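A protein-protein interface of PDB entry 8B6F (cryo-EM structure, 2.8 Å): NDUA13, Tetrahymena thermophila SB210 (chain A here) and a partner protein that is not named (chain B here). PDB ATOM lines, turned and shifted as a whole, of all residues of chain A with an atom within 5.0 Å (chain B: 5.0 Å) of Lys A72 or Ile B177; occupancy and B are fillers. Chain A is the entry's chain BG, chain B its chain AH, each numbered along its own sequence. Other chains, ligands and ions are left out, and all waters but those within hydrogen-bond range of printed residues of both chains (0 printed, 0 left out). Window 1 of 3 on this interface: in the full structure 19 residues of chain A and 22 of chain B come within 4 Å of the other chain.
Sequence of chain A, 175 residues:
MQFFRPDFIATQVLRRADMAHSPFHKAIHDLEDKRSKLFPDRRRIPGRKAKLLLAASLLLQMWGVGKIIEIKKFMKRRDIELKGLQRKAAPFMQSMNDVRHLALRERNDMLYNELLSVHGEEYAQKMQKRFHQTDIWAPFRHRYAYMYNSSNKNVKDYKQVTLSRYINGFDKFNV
Among the printed residues, merely in contact across the chains: Lys A72 with Glu B179 (3.2 Å), Lys A72 with Tyr B189 (3.5 Å), Ile A68 with Ile B198 (3.6 Å), Ile A71 with Tyr B189 (3.7 Å), Ile A68 with Ile B177 (3.9 Å) and Ile A68 with Tyr B189 (3.9 Å).
Of chain B, only Ile B177 (3.0 Å), Glu B179 (3.2 Å) and Tyr B189 (3.5 Å) come within 4 Å of Lys A72.
Of chain A, only Ile A68 (3.9 Å) and Lys A72 (3.0 Å) come within 4 Å of Ile B177.
Of the printed residues of chain B, Ile A71 touches Tyr B189.
Of the printed residues of chain A, Ile B198 touches Ile A68.
Of the printed residues of chain A, Tyr B189 touches Ile A68 (3.9 Å), Ile A71 (3.7 Å) and Lys A72 (3.5 Å).
Of the printed residues of chain A, Glu B179 touches Lys A72.
Of the printed residues of chain B, Ile A68 touches Ile B177 (3.9 Å), Tyr B189 (3.9 Å) and Ile B198 (3.6 Å).
Ser B178 touches none of the printed residues of chain A.
Asn B173 touches none of the printed residues of chain A.
The nearest printed residue of chain A that does not touch Ile B177 is Ile A69 (7.5 Å).
The backbone carbonyl oxygen of Ile B177 is in hydrogen-bond range of the side-chain amino group of Lys A72, 3.0 Å away.
Of the 9 printed residues of chain A, 3 touch a printed residue of chain B.
Hydrophobic or aromatic side chains of chain A that line the printed part of chain B: Ile A68 and Ile A71.
Hydrophobic or aromatic side chains of chain B within 4 Å of the printed part of chain A: Ile B177, Tyr B189 and Ile B198.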
ATOM      1  N   ILE A  68     -17.046  -6.067  -1.514  1.00  0.00           N
ATOM      2  CA  ILE A  68     -16.382  -4.824  -1.898  1.00  0.00           C
ATOM      3  C   ILE A  68     -15.235  -5.110  -2.856  1.00  0.00           C
ATOM      4  O   ILE A  68     -14.999  -4.356  -3.808  1.00  0.00           O
ATOM      5  CB  ILE A  68     -15.902  -4.065  -0.646  1.00  0.00           C
ATOM      6  CG1 ILE A  68     -17.091  -3.603   0.204  1.00  0.00           C
ATOM      7  CG2 ILE A  68     -15.033  -2.871  -1.033  1.00  0.00           C
ATOM      8  CD1 ILE A  68     -18.024  -2.625  -0.477  1.00  0.00           C
ATOM      9  N   ILE A  69     -14.495  -6.194  -2.621  1.00  0.00           N
ATOM     10  CA  ILE A  69     -13.426  -6.564  -3.542  1.00  0.00           C
ATOM     11  C   ILE A  69     -14.011  -6.937  -4.897  1.00  0.00           C
ATOM     12  O   ILE A  69     -13.429  -6.631  -5.943  1.00  0.00           O
ATOM     13  CB  ILE A  69     -12.576  -7.704  -2.951  1.00  0.00           C
ATOM     14  CG1 ILE A  69     -11.847  -7.237  -1.687  1.00  0.00           C
ATOM     15  CG2 ILE A  69     -11.575  -8.224  -3.980  1.00  0.00           C
ATOM     16  CD1 ILE A  69     -10.861  -6.109  -1.899  1.00  0.00           C
ATOM     17  N   GLU A  70     -15.164  -7.606  -4.903  1.00  0.00           N
ATOM     18  CA  GLU A  70     -15.825  -7.917  -6.165  1.00  0.00           C
ATOM     19  C   GLU A  70     -16.177  -6.641  -6.917  1.00  0.00           C
ATOM     20  O   GLU A  70     -15.978  -6.551  -8.133  1.00  0.00           O
ATOM     21  CB  GLU A  70     -17.079  -8.750  -5.900  1.00  0.00           C
ATOM     22  CG  GLU A  70     -17.812  -9.215  -7.151  1.00  0.00           C
ATOM     23  CD  GLU A  70     -17.095 -10.341  -7.872  1.00  0.00           C
ATOM     24  OE1 GLU A  70     -16.404 -11.137  -7.201  1.00  0.00           O
ATOM     25  OE2 GLU A  70     -17.223 -10.430  -9.112  1.00  0.00           O
ATOM     26  N   ILE A  71     -16.719  -5.646  -6.210  1.00  0.00           N
ATOM     27  CA  ILE A  71     -17.061  -4.378  -6.847  1.00  0.00           C
ATOM     28  C   ILE A  71     -15.812  -3.701  -7.393  1.00  0.00           C
ATOM     29  O   ILE A  71     -15.808  -3.188  -8.518  1.00  0.00           O
ATOM     30  CB  ILE A  71     -17.806  -3.468  -5.852  1.00  0.00           C
ATOM     31  CG1 ILE A  71     -19.126  -4.113  -5.432  1.00  0.00           C
ATOM     32  CG2 ILE A  71     -18.071  -2.101  -6.469  1.00  0.00           C
ATOM     33  CD1 ILE A  71     -19.797  -3.431  -4.260  1.00  0.00           C
ATOM     34  N   LYS A  72     -14.733  -3.687  -6.608  1.00  0.00           N
ATOM     35  CA  LYS A  72     -13.497  -3.060  -7.064  1.00  0.00           C
ATOM     36  C   LYS A  72     -12.951  -3.744  -8.308  1.00  0.00           C
ATOM     37  O   LYS A  72     -12.482  -3.079  -9.237  1.00  0.00           O
ATOM     38  CB  LYS A  72     -12.455  -3.082  -5.947  1.00  0.00           C
ATOM     39  CG  LYS A  72     -12.674  -2.039  -4.865  1.00  0.00           C
ATOM     40  CD  LYS A  72     -11.517  -2.029  -3.874  1.00  0.00           C
ATOM     41  CE  LYS A  72     -11.592  -0.835  -2.936  1.00  0.00           C
ATOM     42  NZ  LYS A  72     -12.801  -0.873  -2.073  1.00  0.00           N
ATOM     43  N   LYS A  73     -12.998  -5.076  -8.345  1.00  0.00           N
ATOM     44  CA  LYS A  73     -12.483  -5.793  -9.505  1.00  0.00           C
ATOM     45  C   LYS A  73     -13.354  -5.579 -10.734  1.00  0.00           C
ATOM     46  O   LYS A  73     -12.836  -5.523 -11.854  1.00  0.00           O
ATOM     47  CB  LYS A  73     -12.355  -7.280  -9.182  1.00  0.00           C
ATOM     48  CG  LYS A  73     -11.341  -7.574  -8.087  1.00  0.00           C
ATOM     49  CD  LYS A  73      -9.917  -7.318  -8.551  1.00  0.00           C
ATOM     50  CE  LYS A  73      -8.919  -7.685  -7.466  1.00  0.00           C
ATOM     51  NZ  LYS A  73      -7.515  -7.476  -7.911  1.00  0.00           N
ATOM     52  N   PHE A  74     -14.673  -5.464 -10.555  1.00  0.00           N
ATOM     53  CA  PHE A  74     -15.531  -5.100 -11.677  1.00  0.00           C
ATOM     54  C   PHE A  74     -15.190  -3.708 -12.191  1.00  0.00           C
ATOM     55  O   PHE A  74     -15.135  -3.481 -13.405  1.00  0.00           O
ATOM     56  CB  PHE A  74     -16.999  -5.175 -11.255  1.00  0.00           C
ATOM     57  CG  PHE A  74     -17.965  -4.901 -12.369  1.00  0.00           C
ATOM     58  CD1 PHE A  74     -18.282  -5.888 -13.288  1.00  0.00           C
ATOM     59  CD2 PHE A  74     -18.570  -3.661 -12.490  1.00  0.00           C
ATOM     60  CE1 PHE A  74     -19.177  -5.640 -14.312  1.00  0.00           C
ATOM     61  CE2 PHE A  74     -19.465  -3.407 -13.511  1.00  0.00           C
ATOM     62  CZ  PHE A  74     -19.769  -4.397 -14.423  1.00  0.00           C
ATOM     63  N   MET A  75     -14.959  -2.762 -11.281  1.00  0.00           N
ATOM     64  CA  MET A  75     -14.543  -1.425 -11.691  1.00  0.00           C
ATOM     65  C   MET A  75     -13.241  -1.479 -12.478  1.00  0.00           C
ATOM     66  O   MET A  75     -13.089  -0.791 -13.493  1.00  0.00           O
ATOM     67  CB  MET A  75     -14.387  -0.527 -10.465  1.00  0.00           C
ATOM     68  CG  MET A  75     -15.697  -0.171  -9.785  1.00  0.00           C
ATOM     69  SD  MET A  75     -15.436   0.773  -8.271  1.00  0.00           S
ATOM     70  CE  MET A  75     -17.118   1.193  -7.833  1.00  0.00           C
ATOM     71  N   LYS A  76     -12.294  -2.305 -12.030  1.00  0.00           N
ATOM     72  CA  LYS A  76     -11.028  -2.453 -12.739  1.00  0.00           C
ATOM     73  C   LYS A  76     -11.235  -3.083 -14.110  1.00  0.00           C
ATOM     74  O   LYS A  76     -10.570  -2.702 -15.080  1.00  0.00           O
ATOM     75  CB  LYS A  76     -10.058  -3.286 -11.901  1.00  0.00           C
ATOM     76  CG  LYS A  76      -8.653  -3.365 -12.479  1.00  0.00           C
ATOM     77  CD  LYS A  76      -7.718  -4.169 -11.585  1.00  0.00           C
ATOM     78  CE  LYS A  76      -7.439  -3.453 -10.272  1.00  0.00           C
ATOM     79  NZ  LYS A  76      -6.433  -4.179  -9.447  1.00  0.00           N
ATOM     80  N   ASN B 173     -10.622   3.078   9.524  1.00  0.00           N
ATOM     81  CA  ASN B 173     -11.301   1.885   9.032  1.00  0.00           C
ATOM     82  C   ASN B 173     -12.107   2.184   7.773  1.00  0.00           C
ATOM     83  O   ASN B 173     -12.173   1.352   6.861  1.00  0.00           O
ATOM     84  CB  ASN B 173     -12.201   1.310  10.123  1.00  0.00           C
ATOM     85  CG  ASN B 173     -11.413   0.696  11.262  1.00  0.00           C
ATOM     86  OD1 ASN B 173     -10.274   1.079  11.519  1.00  0.00           O
ATOM     87  ND2 ASN B 173     -12.017  -0.263  11.951  1.00  0.00           N
ATOM     88  N   LEU B 174     -12.730   3.363   7.705  1.00  0.00           N
ATOM     89  CA  LEU B 174     -13.584   3.682   6.564  1.00  0.00           C
ATOM     90  C   LEU B 174     -12.765   3.940   5.304  1.00  0.00           C
ATOM     91  O   LEU B 174     -13.096   3.436   4.226  1.00  0.00           O
ATOM     92  CB  LEU B 174     -14.463   4.890   6.890  1.00  0.00           C
ATOM     93  CG  LEU B 174     -15.574   4.649   7.913  1.00  0.00           C
ATOM     94  CD1 LEU B 174     -16.264   5.955   8.267  1.00  0.00           C
ATOM     95  CD2 LEU B 174     -16.586   3.637   7.402  1.00  0.00           C
ATOM     96  N   ILE B 175     -11.691   4.725   5.416  1.00  0.00           N
ATOM     97  CA  ILE B 175     -10.890   5.055   4.241  1.00  0.00           C
ATOM     98  C   ILE B 175     -10.254   3.814   3.641  1.00  0.00           C
ATOM     99  O   ILE B 175      -9.887   3.814   2.461  1.00  0.00           O
ATOM    100  CB  ILE B 175      -9.806   6.096   4.584  1.00  0.00           C
ATOM    101  CG1 ILE B 175      -8.845   5.529   5.637  1.00  0.00           C
ATOM    102  CG2 ILE B 175     -10.461   7.402   5.026  1.00  0.00           C
ATOM    103  CD1 ILE B 175      -7.780   6.495   6.099  1.00  0.00           C
ATOM    104  N   PHE B 176     -10.098   2.754   4.433  1.00  0.00           N
ATOM    105  CA  PHE B 176      -9.533   1.515   3.921  1.00  0.00           C
ATOM    106  C   PHE B 176     -10.355   0.934   2.779  1.00  0.00           C
ATOM    107  O   PHE B 176      -9.825   0.149   1.986  1.00  0.00           O
ATOM    108  CB  PHE B 176      -9.408   0.505   5.060  1.00  0.00           C
ATOM    109  CG  PHE B 176      -8.883  -0.824   4.628  1.00  0.00           C
ATOM    110  CD1 PHE B 176      -7.633  -0.931   4.044  1.00  0.00           C
ATOM    111  CD2 PHE B 176      -9.626  -1.972   4.832  1.00  0.00           C
ATOM    112  CE1 PHE B 176      -7.146  -2.153   3.648  1.00  0.00           C
ATOM    113  CE2 PHE B 176      -9.144  -3.198   4.442  1.00  0.00           C
ATOM    114  CZ  PHE B 176      -7.899  -3.292   3.851  1.00  0.00           C
ATOM    115  N   ILE B 177     -11.630   1.304   2.673  1.00  0.00           N
ATOM    116  CA  ILE B 177     -12.492   0.834   1.596  1.00  0.00           C
ATOM    117  C   ILE B 177     -12.606   1.922   0.536  1.00  0.00           C
ATOM    118  O   ILE B 177     -12.295   1.696  -0.638  1.00  0.00           O
ATOM    119  CB  ILE B 177     -13.879   0.426   2.128  1.00  0.00           C
ATOM    120  CG1 ILE B 177     -13.826  -0.939   2.826  1.00  0.00           C
ATOM    121  CG2 ILE B 177     -14.913   0.393   1.008  1.00  0.00           C
ATOM    122  CD1 ILE B 177     -13.034  -0.970   4.117  1.00  0.00           C
ATOM    123  N   SER B 178     -13.061   3.108   0.943  1.00  0.00           N
ATOM    124  CA  SER B 178     -13.282   4.187  -0.014  1.00  0.00           C
ATOM    125  C   SER B 178     -11.981   4.621  -0.677  1.00  0.00           C
ATOM    126  O   SER B 178     -11.948   4.870  -1.887  1.00  0.00           O
ATOM    127  CB  SER B 178     -13.940   5.375   0.682  1.00  0.00           C
ATOM    128  OG  SER B 178     -13.090   5.894   1.687  1.00  0.00           O
ATOM    129  N   GLU B 179     -10.904   4.732   0.102  1.00  0.00           N
ATOM    130  CA  GLU B 179      -9.602   5.197  -0.366  1.00  0.00           C
ATOM    131  C   GLU B 179      -9.584   6.694  -0.659  1.00  0.00           C
ATOM    132  O   GLU B 179      -8.751   7.161  -1.438  1.00  0.00           O
ATOM    133  CB  GLU B 179      -9.148   4.428  -1.614  1.00  0.00           C
ATOM    134  CG  GLU B 179      -9.199   2.916  -1.466  1.00  0.00           C
ATOM    135  CD  GLU B 179      -8.784   2.195  -2.735  1.00  0.00           C
ATOM    136  OE1 GLU B 179      -8.349   2.874  -3.688  1.00  0.00           O
ATOM    137  OE2 GLU B 179      -8.898   0.953  -2.783  1.00  0.00           O
ATOM    138  N   TYR B 189     -19.442   2.577  -3.683  1.00  0.00           N
ATOM    139  CA  TYR B 189     -19.246   1.249  -3.113  1.00  0.00           C
ATOM    140  C   TYR B 189     -20.478   0.757  -2.366  1.00  0.00           C
ATOM    141  O   TYR B 189     -20.730  -0.451  -2.329  1.00  0.00           O
ATOM    142  CB  TYR B 189     -18.042   1.253  -2.171  1.00  0.00           C
ATOM    143  CG  TYR B 189     -16.726   1.488  -2.873  1.00  0.00           C
ATOM    144  CD1 TYR B 189     -16.141   0.493  -3.642  1.00  0.00           C
ATOM    145  CD2 TYR B 189     -16.065   2.702  -2.760  1.00  0.00           C
ATOM    146  CE1 TYR B 189     -14.939   0.700  -4.284  1.00  0.00           C
ATOM    147  CE2 TYR B 189     -14.861   2.923  -3.399  1.00  0.00           C
ATOM    148  CZ  TYR B 189     -14.303   1.917  -4.159  1.00  0.00           C
ATOM    149  OH  TYR B 189     -13.103   2.130  -4.797  1.00  0.00           O
ATOM    150  N   LEU B 195     -22.333   0.087   3.678  1.00  0.00           N
ATOM    151  CA  LEU B 195     -21.068  -0.221   4.331  1.00  0.00           C
ATOM    152  C   LEU B 195     -21.241  -0.627   5.786  1.00  0.00           C
ATOM    153  O   LEU B 195     -20.294  -1.152   6.379  1.00  0.00           O
ATOM    154  CB  LEU B 195     -20.126   0.980   4.246  1.00  0.00           C
ATOM    155  CG  LEU B 195     -18.713   0.685   3.744  1.00  0.00           C
ATOM    156  CD1 LEU B 195     -18.742   0.258   2.285  1.00  0.00           C
ATOM    157  CD2 LEU B 195     -17.815   1.897   3.933  1.00  0.00           C
ATOM    158  N   ILE B 198     -20.391  -4.424   6.781  1.00  0.00           N
ATOM    159  CA  ILE B 198     -19.026  -4.806   7.126  1.00  0.00           C
ATOM    160  C   ILE B 198     -18.761  -4.522   8.598  1.00  0.00           C
ATOM    161  O   ILE B 198     -18.074  -5.290   9.280  1.00  0.00           O
ATOM    162  CB  ILE B 198     -18.020  -4.076   6.218  1.00  0.00           C
ATOM    163  CG1 ILE B 198     -18.220  -4.504   4.764  1.00  0.00           C
ATOM    164  CG2 ILE B 198     -16.587  -4.356   6.665  1.00  0.00           C
ATOM    165  CD1 ILE B 198     -17.432  -3.688   3.768  1.00  0.00           C
